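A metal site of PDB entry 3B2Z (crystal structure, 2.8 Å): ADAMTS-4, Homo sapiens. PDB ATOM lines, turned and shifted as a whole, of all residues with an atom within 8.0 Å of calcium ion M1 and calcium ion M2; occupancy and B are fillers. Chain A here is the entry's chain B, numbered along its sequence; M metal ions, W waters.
The side-chain sulfur (SG) of Cys 211 is disulfide-bonded to the side-chain sulfur (SG) of Cys 127, 2.0 Å away.
O of Glu 9 sits at hydrogen-bond distance from N of Thr 100, at 3.4 Å.
Four residues have an atom within 4 Å of calcium ion M1: Glu 9, Asp 99, Cys 211 and Asp 214.
The nearest printed residue that does not touch calcium ion M1 is Leu 212 (4.4 Å).
Of the 26 residues printed, 3 come within 4 Å of calcium ion M2.
Along chain A the residues within 4 Å of calcium ion M2 span positions 9 to 214.
The nearest printed residue that does not touch calcium ion M2 is His 97 (4.3 Å).
Calcium ion M1 is bound by the backbone carbonyl oxygen (O) of Cys 211 (2.2 Å), water W2 (2.2 Å), the side-chain carboxylate (OE1) of Glu 9 (2.3 Å), the side-chain carboxylate (OD1) of Asp 99 (2.4 Å), the side-chain carboxylate (OD1) of Asp 214 (2.5 Å) and the side-chain carboxylate (OD2) of Asp 99 (2.8 Å).
Calcium ion M1 has six donor atoms within binding distance.
Slightly farther from calcium ion M1 lies water W3 (3.0 Å).
Calcium ion M2 is bound by O of Asp 92 (2.3 Å), OD2 of Asp 214 (2.3 Å), OE2 of Glu 9 (2.3 Å), water W2 (2.8 Å) and water W1 (2.9 Å).
Calcium ion M2 has five donor atoms within binding distance.
Slightly farther from calcium ion M2 lies the side-chain carboxylate (OE1) of Glu 9 (2.9 Å).
Water W3 lies within hydrogen-bond range of the backbone carbonyl oxygen (O) of Phe 7 (2.6 Å) and the backbone carbonyl oxygen (O) of Asp 214 (2.7 Å).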
ATOM      1  N   PHE A   7       6.559  14.482 -24.663  1.00  0.00           N
ATOM      2  CA  PHE A   7       7.893  15.071 -24.627  1.00  0.00           C
ATOM      3  C   PHE A   7       8.555  14.979 -25.997  1.00  0.00           C
ATOM      4  O   PHE A   7       8.651  13.898 -26.566  1.00  0.00           O
ATOM      5  CB  PHE A   7       8.772  14.367 -23.580  1.00  0.00           C
ATOM      6  CG  PHE A   7       8.171  14.305 -22.203  1.00  0.00           C
ATOM      7  CD1 PHE A   7       7.289  13.283 -21.845  1.00  0.00           C
ATOM      8  CD2 PHE A   7       8.512  15.250 -21.238  1.00  0.00           C
ATOM      9  CE1 PHE A   7       6.735  13.221 -20.553  1.00  0.00           C
ATOM     10  CE2 PHE A   7       7.967  15.197 -19.943  1.00  0.00           C
ATOM     11  CZ  PHE A   7       7.078  14.181 -19.607  1.00  0.00           C
ATOM     12  N   VAL A   8       9.007  16.122 -26.498  1.00  0.00           N
ATOM     13  CA  VAL A   8       9.683  16.185 -27.793  1.00  0.00           C
ATOM     14  C   VAL A   8      11.213  16.247 -27.654  1.00  0.00           C
ATOM     15  O   VAL A   8      11.799  17.321 -27.582  1.00  0.00           O
ATOM     16  CB  VAL A   8       9.177  17.387 -28.617  1.00  0.00           C
ATOM     17  CG1 VAL A   8       9.722  17.334 -30.024  1.00  0.00           C
ATOM     18  CG2 VAL A   8       7.675  17.381 -28.656  1.00  0.00           C
ATOM     19  N   GLU A   9      11.850  15.082 -27.630  1.00  0.00           N
ATOM     20  CA  GLU A   9      13.311  15.001 -27.550  1.00  0.00           C
ATOM     21  C   GLU A   9      13.978  15.669 -28.757  1.00  0.00           C
ATOM     22  O   GLU A   9      14.073  15.086 -29.835  1.00  0.00           O
ATOM     23  CB  GLU A   9      13.754  13.546 -27.394  1.00  0.00           C
ATOM     24  CG  GLU A   9      13.302  12.930 -26.072  1.00  0.00           C
ATOM     25  CD  GLU A   9      13.103  11.420 -26.133  1.00  0.00           C
ATOM     26  OE1 GLU A   9      12.145  10.967 -26.817  1.00  0.00           O
ATOM     27  OE2 GLU A   9      13.885  10.676 -25.507  1.00  0.00           O
ATOM     28  N   THR A  55      17.779  17.480 -26.044  1.00  0.00           N
ATOM     29  CA  THR A  55      18.538  16.325 -25.547  1.00  0.00           C
ATOM     30  C   THR A  55      19.930  16.260 -26.156  1.00  0.00           C
ATOM     31  O   THR A  55      20.811  15.604 -25.607  1.00  0.00           O
ATOM     32  CB  THR A  55      17.805  14.967 -25.772  1.00  0.00           C
ATOM     33  OG1 THR A  55      17.606  14.718 -27.173  1.00  0.00           O
ATOM     34  CG2 THR A  55      16.446  14.952 -25.057  1.00  0.00           C
ATOM     35  N   ASN A  88      20.836   9.908 -35.728  1.00  0.00           N
ATOM     36  CA  ASN A  88      19.778   9.315 -34.919  1.00  0.00           C
ATOM     37  C   ASN A  88      19.914   7.808 -34.708  1.00  0.00           C
ATOM     38  O   ASN A  88      20.165   7.058 -35.659  1.00  0.00           O
ATOM     39  CB  ASN A  88      18.397   9.645 -35.485  1.00  0.00           C
ATOM     40  CG  ASN A  88      17.372   9.861 -34.397  1.00  0.00           C
ATOM     41  OD1 ASN A  88      17.600   9.490 -33.243  1.00  0.00           O
ATOM     42  ND2 ASN A  88      16.256  10.474 -34.746  1.00  0.00           N
ATOM     43  N   THR A  89      19.755   7.379 -33.454  1.00  0.00           N
ATOM     44  CA  THR A  89      19.902   5.983 -33.068  1.00  0.00           C
ATOM     45  C   THR A  89      18.668   5.189 -33.476  1.00  0.00           C
ATOM     46  O   THR A  89      17.570   5.735 -33.456  1.00  0.00           O
ATOM     47  CB  THR A  89      20.117   5.831 -31.554  1.00  0.00           C
ATOM     48  OG1 THR A  89      18.867   5.999 -30.875  1.00  0.00           O
ATOM     49  CG2 THR A  89      21.123   6.868 -31.046  1.00  0.00           C
ATOM     50  N   GLU A  91      16.780   2.888 -32.069  1.00  0.00           N
ATOM     51  CA  GLU A  91      15.693   2.678 -31.111  1.00  0.00           C
ATOM     52  C   GLU A  91      15.353   3.908 -30.260  1.00  0.00           C
ATOM     53  O   GLU A  91      16.219   4.709 -29.918  1.00  0.00           O
ATOM     54  CB  GLU A  91      15.946   1.450 -30.221  1.00  0.00           C
ATOM     55  CG  GLU A  91      14.671   0.634 -29.951  1.00  0.00           C
ATOM     56  CD  GLU A  91      14.777  -0.340 -28.764  1.00  0.00           C
ATOM     57  OE1 GLU A  91      15.782  -1.085 -28.686  1.00  0.00           O
ATOM     58  OE2 GLU A  91      13.837  -0.367 -27.934  1.00  0.00           O
ATOM     59  N   ASP A  92      14.073   4.019 -29.908  1.00  0.00           N
ATOM     60  CA  ASP A  92      13.509   5.128 -29.123  1.00  0.00           C
ATOM     61  C   ASP A  92      14.088   5.331 -27.713  1.00  0.00           C
ATOM     62  O   ASP A  92      13.925   6.396 -27.126  1.00  0.00           O
ATOM     63  CB  ASP A  92      11.974   4.985 -29.033  1.00  0.00           C
ATOM     64  CG  ASP A  92      11.537   3.731 -28.246  1.00  0.00           C
ATOM     65  OD1 ASP A  92      12.031   2.604 -28.536  1.00  0.00           O
ATOM     66  OD2 ASP A  92      10.655   3.862 -27.346  1.00  0.00           O
ATOM     67  N   SER A  93      14.740   4.307 -27.184  1.00  0.00           N
ATOM     68  CA  SER A  93      15.146   4.293 -25.783  1.00  0.00           C
ATOM     69  C   SER A  93      16.574   4.745 -25.549  1.00  0.00           C
ATOM     70  O   SER A  93      16.882   5.301 -24.491  1.00  0.00           O
ATOM     71  CB  SER A  93      14.963   2.896 -25.214  1.00  0.00           C
ATOM     72  OG  SER A  93      15.594   1.941 -26.046  1.00  0.00           O
ATOM     73  N   ASP A  94      17.446   4.491 -26.518  1.00  0.00           N
ATOM     74  CA  ASP A  94      18.847   4.905 -26.434  1.00  0.00           C
ATOM     75  C   ASP A  94      18.883   6.406 -26.121  1.00  0.00           C
ATOM     76  O   ASP A  94      18.226   7.188 -26.805  1.00  0.00           O
ATOM     77  CB  ASP A  94      19.591   4.607 -27.740  1.00  0.00           C
ATOM     78  CG  ASP A  94      21.103   4.776 -27.606  1.00  0.00           C
ATOM     79  OD1 ASP A  94      21.745   3.913 -26.958  1.00  0.00           O
ATOM     80  OD2 ASP A  94      21.649   5.765 -28.155  1.00  0.00           O
ATOM     81  N   PRO A  95      19.644   6.802 -25.081  1.00  0.00           N
ATOM     82  CA  PRO A  95      19.624   8.188 -24.615  1.00  0.00           C
ATOM     83  C   PRO A  95      19.944   9.242 -25.691  1.00  0.00           C
ATOM     84  O   PRO A  95      19.684  10.421 -25.494  1.00  0.00           O
ATOM     85  CB  PRO A  95      20.697   8.205 -23.514  1.00  0.00           C
ATOM     86  CG  PRO A  95      20.782   6.808 -23.056  1.00  0.00           C
ATOM     87  CD  PRO A  95      20.580   5.987 -24.287  1.00  0.00           C
ATOM     88  N   ASP A  96      20.498   8.793 -26.822  1.00  0.00           N
ATOM     89  CA  ASP A  96      20.900   9.696 -27.901  1.00  0.00           C
ATOM     90  C   ASP A  96      19.889   9.766 -29.068  1.00  0.00           C
ATOM     91  O   ASP A  96      20.144  10.454 -30.062  1.00  0.00           O
ATOM     92  CB  ASP A  96      22.312   9.334 -28.395  1.00  0.00           C
ATOM     93  CG  ASP A  96      23.389   9.544 -27.317  1.00  0.00           C
ATOM     94  OD1 ASP A  96      23.386  10.605 -26.655  1.00  0.00           O
ATOM     95  OD2 ASP A  96      24.249   8.647 -27.149  1.00  0.00           O
ATOM     96  N   HIS A  97      18.765   9.065 -28.937  1.00  0.00           N
ATOM     97  CA  HIS A  97      17.672   9.158 -29.919  1.00  0.00           C
ATOM     98  C   HIS A  97      16.979  10.512 -29.791  1.00  0.00           C
ATOM     99  O   HIS A  97      16.964  11.103 -28.715  1.00  0.00           O
ATOM    100  CB  HIS A  97      16.645   8.041 -29.721  1.00  0.00           C
ATOM    101  CG  HIS A  97      15.636   7.939 -30.827  1.00  0.00           C
ATOM    102  ND1 HIS A  97      15.702   7.343 -32.039  1.00  0.00           N
ATOM    103  CD2 HIS A  97      14.387   8.521 -30.760  1.00  0.00           C
ATOM    104  CE1 HIS A  97      14.501   7.565 -32.665  1.00  0.00           C
ATOM    105  NE2 HIS A  97      13.727   8.279 -31.872  1.00  0.00           N
ATOM    106  N   PHE A  98      16.407  11.004 -30.896  1.00  0.00           N
ATOM    107  CA  PHE A  98      15.619  12.241 -30.861  1.00  0.00           C
ATOM    108  C   PHE A  98      14.368  12.179 -31.737  1.00  0.00           C
ATOM    109  O   PHE A  98      14.340  11.492 -32.769  1.00  0.00           O
ATOM    110  CB  PHE A  98      16.476  13.487 -31.182  1.00  0.00           C
ATOM    111  CG  PHE A  98      17.288  13.363 -32.431  1.00  0.00           C
ATOM    112  CD1 PHE A  98      16.718  13.603 -33.682  1.00  0.00           C
ATOM    113  CD2 PHE A  98      18.640  13.022 -32.367  1.00  0.00           C
ATOM    114  CE1 PHE A  98      17.483  13.480 -34.846  1.00  0.00           C
ATOM    115  CE2 PHE A  98      19.399  12.911 -33.526  1.00  0.00           C
ATOM    116  CZ  PHE A  98      18.820  13.135 -34.764  1.00  0.00           C
ATOM    117  N   ASP A  99      13.338  12.909 -31.324  1.00  0.00           N
ATOM    118  CA  ASP A  99      12.061  12.947 -32.010  1.00  0.00           C
ATOM    119  C   ASP A  99      11.988  14.047 -33.065  1.00  0.00           C
ATOM    120  O   ASP A  99      11.121  14.008 -33.943  1.00  0.00           O
ATOM    121  CB  ASP A  99      10.937  13.104 -31.001  1.00  0.00           C
ATOM    122  CG  ASP A  99      10.996  12.078 -29.877  1.00  0.00           C
ATOM    123  OD1 ASP A  99      11.220  10.878 -30.168  1.00  0.00           O
ATOM    124  OD2 ASP A  99      10.813  12.459 -28.708  1.00  0.00           O
ATOM    125  N   THR A 100      12.877  15.045 -32.984  1.00  0.00           N
ATOM    126  CA  THR A 100      12.999  16.065 -34.027  1.00  0.00           C
ATOM    127  C   THR A 100      14.326  16.821 -33.999  1.00  0.00           C
ATOM    128  O   THR A 100      14.966  16.921 -32.956  1.00  0.00           O
ATOM    129  CB  THR A 100      11.830  17.080 -33.987  1.00  0.00           C
ATOM    130  OG1 THR A 100      11.793  17.796 -35.228  1.00  0.00           O
ATOM    131  CG2 THR A 100      11.992  18.064 -32.833  1.00  0.00           C
ATOM    132  N   CYS A 127       6.915  12.286 -35.675  1.00  0.00           N
ATOM    133  CA  CYS A 127       7.438  10.960 -35.319  1.00  0.00           C
ATOM    134  C   CYS A 127       7.919  10.140 -36.498  1.00  0.00           C
ATOM    135  O   CYS A 127       8.106   8.922 -36.392  1.00  0.00           O
ATOM    136  CB  CYS A 127       6.414  10.185 -34.500  1.00  0.00           C
ATOM    137  SG  CYS A 127       6.181  10.882 -32.875  1.00  0.00           S
ATOM    138  N   GLY A 209       1.886  11.045 -32.749  1.00  0.00           N
ATOM    139  CA  GLY A 209       2.849  11.399 -31.707  1.00  0.00           C
ATOM    140  C   GLY A 209       3.239  10.220 -30.828  1.00  0.00           C
ATOM    141  O   GLY A 209       3.639  10.401 -29.669  1.00  0.00           O
ATOM    142  N   HIS A 210       3.150   9.015 -31.384  1.00  0.00           N
ATOM    143  CA  HIS A 210       3.519   7.801 -30.677  1.00  0.00           C
ATOM    144  C   HIS A 210       4.927   7.836 -30.072  1.00  0.00           C
ATOM    145  O   HIS A 210       5.208   7.141 -29.101  1.00  0.00           O
ATOM    146  CB  HIS A 210       3.370   6.578 -31.591  1.00  0.00           C
ATOM    147  CG  HIS A 210       4.285   6.583 -32.773  1.00  0.00           C
ATOM    148  ND1 HIS A 210       3.923   7.116 -33.988  1.00  0.00           N
ATOM    149  CD2 HIS A 210       5.537   6.090 -32.931  1.00  0.00           C
ATOM    150  CE1 HIS A 210       4.919   6.968 -34.850  1.00  0.00           C
ATOM    151  NE2 HIS A 210       5.913   6.334 -34.235  1.00  0.00           N
ATOM    152  N   CYS A 211       5.799   8.672 -30.644  1.00  0.00           N
ATOM    153  CA  CYS A 211       7.193   8.715 -30.239  1.00  0.00           C
ATOM    154  C   CYS A 211       7.459   9.727 -29.116  1.00  0.00           C
ATOM    155  O   CYS A 211       8.580   9.829 -28.616  1.00  0.00           O
ATOM    156  CB  CYS A 211       8.089   9.001 -31.444  1.00  0.00           C
ATOM    157  SG  CYS A 211       8.010  10.706 -32.000  1.00  0.00           S
ATOM    158  N   LEU A 212       6.412  10.447 -28.714  1.00  0.00           N
ATOM    159  CA  LEU A 212       6.564  11.550 -27.775  1.00  0.00           C
ATOM    160  C   LEU A 212       6.138  11.198 -26.358  1.00  0.00           C
ATOM    161  O   LEU A 212       5.831  12.080 -25.569  1.00  0.00           O
ATOM    162  CB  LEU A 212       5.772  12.764 -28.270  1.00  0.00           C
ATOM    163  CG  LEU A 212       6.003  13.202 -29.715  1.00  0.00           C
ATOM    164  CD1 LEU A 212       5.005  14.276 -30.111  1.00  0.00           C
ATOM    165  CD2 LEU A 212       7.407  13.700 -29.889  1.00  0.00           C
ATOM    166  N   LEU A 213       6.148   9.900 -26.038  1.00  0.00           N
ATOM    167  CA  LEU A 213       5.627   9.434 -24.743  1.00  0.00           C
ATOM    168  C   LEU A 213       6.695   9.058 -23.734  1.00  0.00           C
ATOM    169  O   LEU A 213       6.433   9.093 -22.530  1.00  0.00           O
ATOM    170  CB  LEU A 213       4.622   8.286 -24.936  1.00  0.00           C
ATOM    171  CG  LEU A 213       3.326   8.725 -25.626  1.00  0.00           C
ATOM    172  CD1 LEU A 213       2.713   7.568 -26.379  1.00  0.00           C
ATOM    173  CD2 LEU A 213       2.328   9.339 -24.641  1.00  0.00           C
ATOM    174  N   ASP A 214       7.877   8.692 -24.222  1.00  0.00           N
ATOM    175  CA  ASP A 214       9.010   8.396 -23.342  1.00  0.00           C
ATOM    176  C   ASP A 214       9.677   9.681 -22.850  1.00  0.00           C
ATOM    177  O   ASP A 214      10.102  10.515 -23.640  1.00  0.00           O
ATOM    178  CB  ASP A 214      10.020   7.431 -23.999  1.00  0.00           C
ATOM    179  CG  ASP A 214      10.684   8.012 -25.256  1.00  0.00           C
ATOM    180  OD1 ASP A 214       9.990   8.303 -26.245  1.00  0.00           O
ATOM    181  OD2 ASP A 214      11.930   8.163 -25.257  1.00  0.00           O
ATOM    182  N   LYS A 215       9.733   9.824 -21.533  1.00  0.00           N
ATOM    183  CA  LYS A 215      10.426  10.935 -20.900  1.00  0.00           C
ATOM    184  C   LYS A 215      11.925  10.666 -21.059  1.00  0.00           C
ATOM    185  O   LYS A 215      12.362   9.539 -20.822  1.00  0.00           O
ATOM    186  CB  LYS A 215      10.037  10.997 -19.414  1.00  0.00           C
ATOM    187  CG  LYS A 215      10.360  12.316 -18.695  1.00  0.00           C
ATOM    188  CD  LYS A 215      10.362  12.130 -17.161  1.00  0.00           C
ATOM    189  CE  LYS A 215      11.609  11.364 -16.686  1.00  0.00           C
ATOM    190  NZ  LYS A 215      11.545  10.860 -15.273  1.00  0.00           N
ATOM    191  N   PRO A 216      12.711  11.686 -21.475  1.00  0.00           N
ATOM    192  CA  PRO A 216      14.129  11.481 -21.747  1.00  0.00           C
ATOM    193  C   PRO A 216      14.961  11.470 -20.471  1.00  0.00           C
ATOM    194  O   PRO A 216      14.559  12.079 -19.469  1.00  0.00           O
ATOM    195  CB  PRO A 216      14.493  12.690 -22.582  1.00  0.00           C
ATOM    196  CG  PRO A 216      13.603  13.762 -22.074  1.00  0.00           C
ATOM    197  CD  PRO A 216      12.313  13.084 -21.693  1.00  0.00           C
ATOM    198  N   GLU A 217      16.127  10.819 -20.527  1.00  0.00           N
ATOM    199  CA  GLU A 217      16.968  10.590 -19.347  1.00  0.00           C
ATOM    200  C   GLU A 217      17.628  11.867 -18.815  1.00  0.00           C
ATOM    201  O   GLU A 217      17.261  12.373 -17.751  1.00  0.00           O
ATOM    202  CB  GLU A 217      18.064   9.544 -19.651  1.00  0.00           C
ATOM    203  CG  GLU A 217      17.556   8.119 -19.915  1.00  0.00           C
ATOM    204  CD  GLU A 217      16.816   7.532 -18.723  1.00  0.00           C
ATOM    205  OE1 GLU A 217      17.480   7.070 -17.759  1.00  0.00           O
ATOM    206  OE2 GLU A 217      15.571   7.520 -18.752  1.00  0.00           O
HETATM  207 CA    CA M   1      10.733   9.676 -28.149  1.00  0.00          CA
HETATM  208 CA    CA M   2      13.777   8.579 -26.549  1.00  0.00          CA
HETATM  209  O   HOH W   1      13.807   8.662 -23.678  1.00  0.00           O
HETATM  210  O   HOH W   2      11.917   7.850 -28.522  1.00  0.00           O
HETATM  211  O   HOH W   3       9.572  11.499 -26.101  1.00  0.00           O
